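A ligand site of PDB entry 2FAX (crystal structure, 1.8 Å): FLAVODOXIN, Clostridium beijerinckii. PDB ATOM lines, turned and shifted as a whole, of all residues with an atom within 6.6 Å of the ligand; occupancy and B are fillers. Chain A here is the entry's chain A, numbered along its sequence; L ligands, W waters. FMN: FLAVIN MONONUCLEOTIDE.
O1P of the ligand is in hydrogen-bond range of OG1 of Thr 12 (2.8 Å). A nitrogen (N3) of the ligand is in hydrogen-bond range of the side-chain carboxylate (OE2) of Glu 59 (2.8 Å). An oxygen (O2') of the ligand is in hydrogen-bond range of the backbone carbonyl oxygen (O) of Ala 55 (2.7 Å). OG of Ser 7 lies within hydrogen-bond range of O1P of the ligand (2.7 Å). The backbone NH (N) of Thr 9 lies within hydrogen-bond range of an oxygen (O3P) of the ligand (2.8 Å). The backbone NH of Gly 8 sits at hydrogen-bond distance from an oxygen (O2P) of the ligand (2.7 Å). The backbone NH of Ala 55 lies within hydrogen-bond range of an oxygen (O2') of the ligand, 3.4 Å away. N of Glu 59 is in hydrogen-bond range of O4 of the ligand (2.9 Å). N of Gly 10 lies within hydrogen-bond range of O3P of the ligand. N of Gly 91 lies within hydrogen-bond range of O2 of the ligand, 2.8 Å away. The backbone NH (N) of Trp 90 sits at hydrogen-bond distance from an oxygen (O2) of the ligand (3.4 Å). The backbone NH of Thr 12 lies within hydrogen-bond range of an oxygen (O1P) of the ligand, 2.7 Å away. N of Asn 11 lies within hydrogen-bond range of O3P of the ligand (3.0 Å). O3P of the ligand sits at hydrogen-bond distance from OG1 of Thr 9 (2.6 Å). O4' of the ligand lies within hydrogen-bond range of OD1 of Asn 11, at 2.8 Å. The side-chain hydroxyl (OG) of Ser 54 lies within hydrogen-bond range of an oxygen (O2P) of the ligand. The side-chain hydroxyl (OG) of Ser 87 sits at hydrogen-bond distance from an oxygen (O4') of the ligand, at 2.7 Å. N of Gly 89 sits at hydrogen-bond distance from O2 of the ligand (3.1 Å).
The backbone NH of Ala 55 is in hydrogen-bond range of the backbone carbonyl oxygen of Ser 87 (3.0 Å). The backbone carbonyl oxygen (O) of Ser 54 sits at hydrogen-bond distance from the indole nitrogen (NE1) of Trp 95, at 3.4 Å. N of Thr 12 is in hydrogen-bond range of OG of Ser 7. N of Glu 13 is in hydrogen-bond range of OG of Ser 7, at 3.3 Å. The backbone NH (N) of Ser 54 lies within hydrogen-bond range of the side-chain hydroxyl (OG1) of Thr 12 (3.5 Å). O of Val 117 sits close to OG of Ser 87 (3.2 Å). The side-chain hydroxyl (OG) of Ser 7 sits at hydrogen-bond distance from the backbone NH (N) of Gly 10. The side-chain hydroxyl (OG1) of Thr 12 is in hydrogen-bond range of the backbone NH (N) of Ser 87.
CZ3 of Trp 6 touches O2P of the ligand (3.8 Å). C of Met 56 touches N5 of the ligand (3.4 Å). Gly 57 touches the ligand (N to C6, 3.2 Å). Asp 58 touches the ligand (N to O4, 3.7 Å). Tyr 88 touches the ligand (CA to O2', 3.4 Å). Asn 119 touches the ligand (CA to O4', 3.5 Å). Along chain A the residues within 4 Å of the ligand span positions 6 to 119. The nearest printed residue that does not touch the ligand is Glu 13 (4.5 Å).
Water W5 lies within hydrogen-bond range of an oxygen (O3') of the ligand (2.7 Å), the side-chain amide oxygen of Asn 119 (2.7 Å) and the side-chain amide oxygen of Asn 11 (3.3 Å). Water W4 lies within hydrogen-bond range of OE1 of Glu 59 (2.8 Å), N of Gly 93 (2.9 Å), O2 of the ligand (3.2 Å) and N of Asp 92 (3.5 Å). Water W6 bridges NE1 of Trp 90 and O4 of the ligand.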
ATOM      1  N   TRP A   6      30.493  -3.856   1.852  1.00  0.00           N
ATOM      2  CA  TRP A   6      29.168  -3.718   2.466  1.00  0.00           C
ATOM      3  C   TRP A   6      28.428  -2.746   1.535  1.00  0.00           C
ATOM      4  O   TRP A   6      28.996  -1.731   1.111  1.00  0.00           O
ATOM      5  CB  TRP A   6      29.214  -3.137   3.887  1.00  0.00           C
ATOM      6  CG  TRP A   6      27.820  -3.114   4.500  1.00  0.00           C
ATOM      7  CD1 TRP A   6      27.219  -4.127   5.182  1.00  0.00           C
ATOM      8  CD2 TRP A   6      26.825  -2.082   4.356  1.00  0.00           C
ATOM      9  NE1 TRP A   6      25.907  -3.810   5.460  1.00  0.00           N
ATOM     10  CE2 TRP A   6      25.634  -2.560   4.974  1.00  0.00           C
ATOM     11  CE3 TRP A   6      26.810  -0.813   3.763  1.00  0.00           C
ATOM     12  CZ2 TRP A   6      24.456  -1.811   5.004  1.00  0.00           C
ATOM     13  CZ3 TRP A   6      25.622  -0.070   3.802  1.00  0.00           C
ATOM     14  CH2 TRP A   6      24.471  -0.570   4.417  1.00  0.00           C
ATOM     15  N   SER A   7      27.176  -3.066   1.194  1.00  0.00           N
ATOM     16  CA  SER A   7      26.366  -2.211   0.344  1.00  0.00           C
ATOM     17  C   SER A   7      24.905  -2.250   0.805  1.00  0.00           C
ATOM     18  O   SER A   7      24.330  -3.323   0.994  1.00  0.00           O
ATOM     19  CB  SER A   7      26.472  -2.665  -1.113  1.00  0.00           C
ATOM     20  OG  SER A   7      25.823  -1.758  -1.976  1.00  0.00           O
ATOM     21  N   GLY A   8      24.306  -1.081   0.993  1.00  0.00           N
ATOM     22  CA  GLY A   8      22.934  -1.015   1.457  1.00  0.00           C
ATOM     23  C   GLY A   8      21.875  -0.977   0.373  1.00  0.00           C
ATOM     24  O   GLY A   8      20.724  -1.347   0.621  1.00  0.00           O
ATOM     25  N   THR A   9      22.229  -0.478  -0.801  1.00  0.00           N
ATOM     26  CA  THR A   9      21.292  -0.415  -1.915  1.00  0.00           C
ATOM     27  C   THR A   9      21.900  -1.041  -3.187  1.00  0.00           C
ATOM     28  O   THR A   9      21.237  -1.140  -4.229  1.00  0.00           O
ATOM     29  CB  THR A   9      20.811   1.050  -2.208  1.00  0.00           C
ATOM     30  OG1 THR A   9      21.825   1.772  -2.933  1.00  0.00           O
ATOM     31  CG2 THR A   9      20.510   1.804  -0.893  1.00  0.00           C
ATOM     32  N   GLY A  10      23.158  -1.462  -3.097  1.00  0.00           N
ATOM     33  CA  GLY A  10      23.823  -2.082  -4.228  1.00  0.00           C
ATOM     34  C   GLY A  10      24.816  -1.211  -4.979  1.00  0.00           C
ATOM     35  O   GLY A  10      25.442  -1.688  -5.926  1.00  0.00           O
ATOM     36  N   ASN A  11      24.997   0.036  -4.572  1.00  0.00           N
ATOM     37  CA  ASN A  11      25.919   0.929  -5.265  1.00  0.00           C
ATOM     38  C   ASN A  11      27.372   0.471  -5.119  1.00  0.00           C
ATOM     39  O   ASN A  11      28.092   0.307  -6.116  1.00  0.00           O
ATOM     40  CB  ASN A  11      25.741   2.384  -4.813  1.00  0.00           C
ATOM     41  CG  ASN A  11      24.413   2.967  -5.254  1.00  0.00           C
ATOM     42  OD1 ASN A  11      23.929   3.928  -4.655  1.00  0.00           O
ATOM     43  ND2 ASN A  11      23.827   2.416  -6.304  1.00  0.00           N
ATOM     44  N   THR A  12      27.781   0.223  -3.874  1.00  0.00           N
ATOM     45  CA  THR A  12      29.123  -0.264  -3.595  1.00  0.00           C
ATOM     46  C   THR A  12      29.272  -1.697  -4.103  1.00  0.00           C
ATOM     47  O   THR A  12      30.344  -2.110  -4.514  1.00  0.00           O
ATOM     48  CB  THR A  12      29.449  -0.173  -2.085  1.00  0.00           C
ATOM     49  OG1 THR A  12      29.324   1.191  -1.673  1.00  0.00           O
ATOM     50  CG2 THR A  12      30.890  -0.647  -1.809  1.00  0.00           C
ATOM     51  N   GLU A  13      28.178  -2.457  -4.113  1.00  0.00           N
ATOM     52  CA  GLU A  13      28.220  -3.816  -4.631  1.00  0.00           C
ATOM     53  C   GLU A  13      28.555  -3.776  -6.137  1.00  0.00           C
ATOM     54  O   GLU A  13      29.391  -4.548  -6.615  1.00  0.00           O
ATOM     55  CB  GLU A  13      26.891  -4.515  -4.410  1.00  0.00           C
ATOM     56  CG  GLU A  13      26.864  -5.945  -4.960  1.00  0.00           C
ATOM     57  CD  GLU A  13      25.501  -6.605  -4.827  1.00  0.00           C
ATOM     58  OE1 GLU A  13      24.472  -5.897  -4.739  1.00  0.00           O
ATOM     59  OE2 GLU A  13      25.456  -7.855  -4.814  1.00  0.00           O
ATOM     60  N   CYS A  53      33.015   0.138   1.291  1.00  0.00           N
ATOM     61  CA  CYS A  53      31.844   0.447   2.113  1.00  0.00           C
ATOM     62  C   CYS A  53      31.378   1.860   1.792  1.00  0.00           C
ATOM     63  O   CYS A  53      32.194   2.770   1.659  1.00  0.00           O
ATOM     64  CB  CYS A  53      32.155   0.361   3.612  1.00  0.00           C
ATOM     65  SG  CYS A  53      30.721   0.599   4.703  1.00  0.00           S
ATOM     66  N   SER A  54      30.073   2.018   1.637  1.00  0.00           N
ATOM     67  CA  SER A  54      29.480   3.319   1.357  1.00  0.00           C
ATOM     68  C   SER A  54      29.534   4.236   2.580  1.00  0.00           C
ATOM     69  O   SER A  54      29.791   3.785   3.721  1.00  0.00           O
ATOM     70  CB  SER A  54      28.019   3.141   0.916  1.00  0.00           C
ATOM     71  OG  SER A  54      27.351   2.268   1.817  1.00  0.00           O
ATOM     72  N   ALA A  55      29.260   5.517   2.337  1.00  0.00           N
ATOM     73  CA  ALA A  55      29.257   6.530   3.387  1.00  0.00           C
ATOM     74  C   ALA A  55      27.948   6.401   4.150  1.00  0.00           C
ATOM     75  O   ALA A  55      26.867   6.490   3.569  1.00  0.00           O
ATOM     76  CB  ALA A  55      29.361   7.940   2.762  1.00  0.00           C
ATOM     77  N   MET A  56      28.050   6.132   5.443  1.00  0.00           N
ATOM     78  CA  MET A  56      26.872   6.002   6.291  1.00  0.00           C
ATOM     79  C   MET A  56      26.817   7.112   7.340  1.00  0.00           C
ATOM     80  O   MET A  56      27.755   7.874   7.485  1.00  0.00           O
ATOM     81  CB  MET A  56      26.820   4.602   6.925  1.00  0.00           C
ATOM     82  CG  MET A  56      26.434   3.506   5.930  1.00  0.00           C
ATOM     83  SD  MET A  56      24.751   3.715   5.249  1.00  0.00           S
ATOM     84  CE  MET A  56      23.817   2.980   6.486  1.00  0.00           C
ATOM     85  N   GLY A  57      25.690   7.184   8.041  1.00  0.00           N
ATOM     86  CA  GLY A  57      25.408   8.215   9.030  1.00  0.00           C
ATOM     87  C   GLY A  57      26.510   9.106   9.558  1.00  0.00           C
ATOM     88  O   GLY A  57      27.344   8.661  10.334  1.00  0.00           O
ATOM     89  N   ASP A  58      26.479  10.381   9.185  1.00  0.00           N
ATOM     90  CA  ASP A  58      27.485  11.331   9.634  1.00  0.00           C
ATOM     91  C   ASP A  58      28.887  10.977   9.179  1.00  0.00           C
ATOM     92  O   ASP A  58      29.839  11.034   9.958  1.00  0.00           O
ATOM     93  CB  ASP A  58      27.467  11.482  11.162  1.00  0.00           C
ATOM     94  CG  ASP A  58      26.480  12.513  11.618  1.00  0.00           C
ATOM     95  OD1 ASP A  58      26.673  13.695  11.278  1.00  0.00           O
ATOM     96  OD2 ASP A  58      25.511  12.137  12.315  1.00  0.00           O
ATOM     97  N   GLU A  59      28.996  10.562   7.915  1.00  0.00           N
ATOM     98  CA  GLU A  59      30.283  10.236   7.318  1.00  0.00           C
ATOM     99  C   GLU A  59      31.089   9.175   8.059  1.00  0.00           C
ATOM    100  O   GLU A  59      32.256   9.404   8.396  1.00  0.00           O
ATOM    101  CB  GLU A  59      31.127  11.510   7.194  1.00  0.00           C
ATOM    102  CG  GLU A  59      30.515  12.604   6.314  1.00  0.00           C
ATOM    103  CD  GLU A  59      30.509  12.255   4.835  1.00  0.00           C
ATOM    104  OE1 GLU A  59      31.253  11.349   4.415  1.00  0.00           O
ATOM    105  OE2 GLU A  59      29.771  12.918   4.083  1.00  0.00           O
ATOM    106  N   VAL A  60      30.498   8.003   8.298  1.00  0.00           N
ATOM    107  CA  VAL A  60      31.233   6.936   8.976  1.00  0.00           C
ATOM    108  C   VAL A  60      31.049   5.640   8.203  1.00  0.00           C
ATOM    109  O   VAL A  60      30.241   5.584   7.277  1.00  0.00           O
ATOM    110  CB  VAL A  60      30.750   6.727  10.437  1.00  0.00           C
ATOM    111  CG1 VAL A  60      30.981   7.976  11.260  1.00  0.00           C
ATOM    112  CG2 VAL A  60      29.257   6.328  10.472  1.00  0.00           C
ATOM    113  N   GLY A  86      34.288   2.906  -2.226  1.00  0.00           N
ATOM    114  CA  GLY A  86      32.931   2.996  -1.739  1.00  0.00           C
ATOM    115  C   GLY A  86      32.127   4.049  -2.459  1.00  0.00           C
ATOM    116  O   GLY A  86      32.693   4.939  -3.104  1.00  0.00           O
ATOM    117  N   SER A  87      30.809   3.923  -2.368  1.00  0.00           N
ATOM    118  CA  SER A  87      29.890   4.883  -2.975  1.00  0.00           C
ATOM    119  C   SER A  87      29.419   5.867  -1.897  1.00  0.00           C
ATOM    120  O   SER A  87      29.390   5.528  -0.698  1.00  0.00           O
ATOM    121  CB  SER A  87      28.681   4.132  -3.555  1.00  0.00           C
ATOM    122  OG  SER A  87      27.754   5.014  -4.172  1.00  0.00           O
ATOM    123  N   TYR A  88      29.096   7.083  -2.311  1.00  0.00           N
ATOM    124  CA  TYR A  88      28.623   8.107  -1.376  1.00  0.00           C
ATOM    125  C   TYR A  88      27.524   8.934  -2.044  1.00  0.00           C
ATOM    126  O   TYR A  88      27.266   8.807  -3.246  1.00  0.00           O
ATOM    127  CB  TYR A  88      29.765   9.005  -0.892  1.00  0.00           C
ATOM    128  CG  TYR A  88      30.386   9.849  -1.974  1.00  0.00           C
ATOM    129  CD1 TYR A  88      31.264   9.294  -2.905  1.00  0.00           C
ATOM    130  CD2 TYR A  88      30.081  11.199  -2.082  1.00  0.00           C
ATOM    131  CE1 TYR A  88      31.832  10.068  -3.903  1.00  0.00           C
ATOM    132  CE2 TYR A  88      30.638  11.990  -3.082  1.00  0.00           C
ATOM    133  CZ  TYR A  88      31.515  11.414  -3.993  1.00  0.00           C
ATOM    134  OH  TYR A  88      32.047  12.188  -4.998  1.00  0.00           O
ATOM    135  N   GLY A  89      26.873   9.768  -1.250  1.00  0.00           N
ATOM    136  CA  GLY A  89      25.785  10.574  -1.763  1.00  0.00           C
ATOM    137  C   GLY A  89      26.070  12.049  -1.848  1.00  0.00           C
ATOM    138  O   GLY A  89      26.762  12.497  -2.758  1.00  0.00           O
ATOM    139  N   TRP A  90      25.560  12.782  -0.865  1.00  0.00           N
ATOM    140  CA  TRP A  90      25.680  14.246  -0.787  1.00  0.00           C
ATOM    141  C   TRP A  90      26.997  14.830  -0.276  1.00  0.00           C
ATOM    142  O   TRP A  90      27.198  16.040  -0.342  1.00  0.00           O
ATOM    143  CB  TRP A  90      24.531  14.797   0.055  1.00  0.00           C
ATOM    144  CG  TRP A  90      24.461  14.195   1.435  1.00  0.00           C
ATOM    145  CD1 TRP A  90      25.157  14.597   2.548  1.00  0.00           C
ATOM    146  CD2 TRP A  90      23.690  13.051   1.844  1.00  0.00           C
ATOM    147  NE1 TRP A  90      24.870  13.782   3.608  1.00  0.00           N
ATOM    148  CE2 TRP A  90      23.971  12.821   3.209  1.00  0.00           C
ATOM    149  CE3 TRP A  90      22.789  12.198   1.189  1.00  0.00           C
ATOM    150  CZ2 TRP A  90      23.393  11.780   3.936  1.00  0.00           C
ATOM    151  CZ3 TRP A  90      22.213  11.157   1.906  1.00  0.00           C
ATOM    152  CH2 TRP A  90      22.513  10.952   3.274  1.00  0.00           C
ATOM    153  N   GLY A  91      27.864  13.998   0.289  1.00  0.00           N
ATOM    154  CA  GLY A  91      29.124  14.500   0.811  1.00  0.00           C
ATOM    155  C   GLY A  91      30.209  14.605  -0.246  1.00  0.00           C
ATOM    156  O   GLY A  91      29.936  14.612  -1.444  1.00  0.00           O
ATOM    157  N   ASP A  92      31.463  14.713   0.189  1.00  0.00           N
ATOM    158  CA  ASP A  92      32.580  14.794  -0.750  1.00  0.00           C
ATOM    159  C   ASP A  92      33.730  13.839  -0.396  1.00  0.00           C
ATOM    160  O   ASP A  92      34.877  14.054  -0.814  1.00  0.00           O
ATOM    161  CB  ASP A  92      33.093  16.227  -0.886  1.00  0.00           C
ATOM    162  CG  ASP A  92      33.601  16.810   0.425  1.00  0.00           C
ATOM    163  OD1 ASP A  92      33.848  16.069   1.396  1.00  0.00           O
ATOM    164  OD2 ASP A  92      33.753  18.050   0.462  1.00  0.00           O
ATOM    165  N   GLY A  93      33.434  12.815   0.381  1.00  0.00           N
ATOM    166  CA  GLY A  93      34.447  11.833   0.731  1.00  0.00           C
ATOM    167  C   GLY A  93      34.995  11.849   2.139  1.00  0.00           C
ATOM    168  O   GLY A  93      35.969  11.138   2.387  1.00  0.00           O
ATOM    169  N   TRP A  95      34.078  10.373   4.916  1.00  0.00           N
ATOM    170  CA  TRP A  95      34.159   9.024   5.492  1.00  0.00           C
ATOM    171  C   TRP A  95      35.360   8.246   4.937  1.00  0.00           C
ATOM    172  O   TRP A  95      35.996   7.468   5.664  1.00  0.00           O
ATOM    173  CB  TRP A  95      32.847   8.244   5.280  1.00  0.00           C
ATOM    174  CG  TRP A  95      32.839   7.206   4.179  1.00  0.00           C
ATOM    175  CD1 TRP A  95      32.799   5.836   4.337  1.00  0.00           C
ATOM    176  CD2 TRP A  95      32.832   7.435   2.761  1.00  0.00           C
ATOM    177  NE1 TRP A  95      32.768   5.219   3.112  1.00  0.00           N
ATOM    178  CE2 TRP A  95      32.785   6.171   2.124  1.00  0.00           C
ATOM    179  CE3 TRP A  95      32.853   8.592   1.963  1.00  0.00           C
ATOM    180  CZ2 TRP A  95      32.751   6.029   0.728  1.00  0.00           C
ATOM    181  CZ3 TRP A  95      32.827   8.455   0.569  1.00  0.00           C
ATOM    182  CH2 TRP A  95      32.783   7.175  -0.027  1.00  0.00           C
ATOM    183  N   VAL A 117      32.820   6.915  -5.624  1.00  0.00           N
ATOM    184  CA  VAL A 117      31.896   7.178  -6.729  1.00  0.00           C
ATOM    185  C   VAL A 117      30.559   7.602  -6.142  1.00  0.00           C
ATOM    186  O   VAL A 117      30.093   7.008  -5.159  1.00  0.00           O
ATOM    187  CB  VAL A 117      31.705   5.914  -7.585  1.00  0.00           C
ATOM    188  CG1 VAL A 117      30.522   6.070  -8.531  1.00  0.00           C
ATOM    189  CG2 VAL A 117      32.994   5.635  -8.376  1.00  0.00           C
ATOM    190  N   GLN A 118      29.952   8.631  -6.725  1.00  0.00           N
ATOM    191  CA  GLN A 118      28.683   9.121  -6.229  1.00  0.00           C
ATOM    192  C   GLN A 118      27.520   8.265  -6.748  1.00  0.00           C
ATOM    193  O   GLN A 118      27.357   8.088  -7.963  1.00  0.00           O
ATOM    194  CB  GLN A 118      28.492  10.576  -6.633  1.00  0.00           C
ATOM    195  CG  GLN A 118      27.267  11.235  -5.969  1.00  0.00           C
ATOM    196  CD  GLN A 118      27.132  12.712  -6.292  1.00  0.00           C
ATOM    197  OE1 GLN A 118      27.980  13.295  -7.004  1.00  0.00           O
ATOM    198  NE2 GLN A 118      26.082  13.343  -5.780  1.00  0.00           N
ATOM    199  N   ASN A 119      26.740   7.741  -5.812  1.00  0.00           N
ATOM    200  CA  ASN A 119      25.558   6.913  -6.111  1.00  0.00           C
ATOM    201  C   ASN A 119      25.941   5.698  -6.987  1.00  0.00           C
ATOM    202  O   ASN A 119      27.014   5.126  -6.796  1.00  0.00           O
ATOM    203  CB  ASN A 119      24.456   7.754  -6.749  1.00  0.00           C
ATOM    204  CG  ASN A 119      24.169   9.030  -5.958  1.00  0.00           C
ATOM    205  OD1 ASN A 119      23.812   8.995  -4.772  1.00  0.00           O
ATOM    206  ND2 ASN A 119      24.378  10.171  -6.600  1.00  0.00           N
ATOM    207  N   GLU A 120      25.065   5.257  -7.888  1.00  0.00           N
ATOM    208  CA  GLU A 120      25.407   4.094  -8.722  1.00  0.00           C
ATOM    209  C   GLU A 120      26.492   4.566  -9.694  1.00  0.00           C
ATOM    210  O   GLU A 120      26.401   5.662 -10.237  1.00  0.00           O
ATOM    211  CB  GLU A 120      24.195   3.565  -9.499  1.00  0.00           C
ATOM    212  CG  GLU A 120      24.461   2.159 -10.088  1.00  0.00           C
ATOM    213  CD  GLU A 120      23.342   1.649 -10.991  1.00  0.00           C
ATOM    214  OE1 GLU A 120      22.160   1.753 -10.595  1.00  0.00           O
ATOM    215  OE2 GLU A 120      23.650   1.107 -12.085  1.00  0.00           O
HETATM  216  N1  FMN L   1      26.418   9.936   1.806  1.00  0.00           N
HETATM  217  C2  FMN L   1      27.378  10.857   2.063  1.00  0.00           C
HETATM  218  O2  FMN L   1      27.985  11.368   1.137  1.00  0.00           O
HETATM  219  N3  FMN L   1      27.658  11.194   3.398  1.00  0.00           N
HETATM  220  C4  FMN L   1      27.029  10.669   4.514  1.00  0.00           C
HETATM  221  O4  FMN L   1      27.317  11.008   5.647  1.00  0.00           O
HETATM  222  C4A FMN L   1      25.973   9.669   4.199  1.00  0.00           C
HETATM  223  N5  FMN L   1      25.270   9.164   5.179  1.00  0.00           N
HETATM  224  C5A FMN L   1      24.236   8.304   4.836  1.00  0.00           C
HETATM  225  C6  FMN L   1      23.414   7.780   5.876  1.00  0.00           C
HETATM  226  C7  FMN L   1      22.417   6.874   5.642  1.00  0.00           C
HETATM  227  C7M FMN L   1      21.579   6.401   6.790  1.00  0.00           C
HETATM  228  C8  FMN L   1      22.198   6.408   4.300  1.00  0.00           C
HETATM  229  C8M FMN L   1      21.209   5.293   3.959  1.00  0.00           C
HETATM  230  C9  FMN L   1      22.934   6.973   3.254  1.00  0.00           C
HETATM  231  C9A FMN L   1      23.970   7.892   3.495  1.00  0.00           C
HETATM  232  N10 FMN L   1      24.734   8.479   2.484  1.00  0.00           N
HETATM  233  C10 FMN L   1      25.745   9.367   2.782  1.00  0.00           C
HETATM  234  C1' FMN L   1      24.424   8.151   1.082  1.00  0.00           C
HETATM  235  C2' FMN L   1      25.050   6.815   0.658  1.00  0.00           C
HETATM  236  O2' FMN L   1      26.449   6.814   0.939  1.00  0.00           O
HETATM  237  C3' FMN L   1      24.832   6.614  -0.851  1.00  0.00           C
HETATM  238  O3' FMN L   1      23.436   6.534  -1.120  1.00  0.00           O
HETATM  239  C4' FMN L   1      25.556   5.428  -1.504  1.00  0.00           C
HETATM  240  O4' FMN L   1      25.398   5.501  -2.925  1.00  0.00           O
HETATM  241  C5' FMN L   1      25.032   4.103  -0.935  1.00  0.00           C
HETATM  242  O5' FMN L   1      25.798   3.013  -1.420  1.00  0.00           O
HETATM  243  P   FMN L   1      25.399   1.550  -1.061  1.00  0.00           P
HETATM  244  O1P FMN L   1      26.532   0.777  -1.516  1.00  0.00           O
HETATM  245  O2P FMN L   1      25.087   1.470   0.389  1.00  0.00           O
HETATM  246  O3P FMN L   1      24.176   1.156  -1.933  1.00  0.00           O
HETATM  247  O   HOH W   1      22.110   4.874   0.571  1.00  0.00           O
HETATM  248  O   HOH W   2      20.726   2.447   5.800  1.00  0.00           O
HETATM  249  O   HOH W   3      22.871   2.396   1.684  1.00  0.00           O
HETATM  250  O   HOH W   4      31.096  11.576   1.599  1.00  0.00           O
HETATM  251  O   HOH W   5      22.627   6.817  -3.636  1.00  0.00           O
HETATM  252  O   HOH W   6      26.007  14.030   6.347  1.00  0.00           O
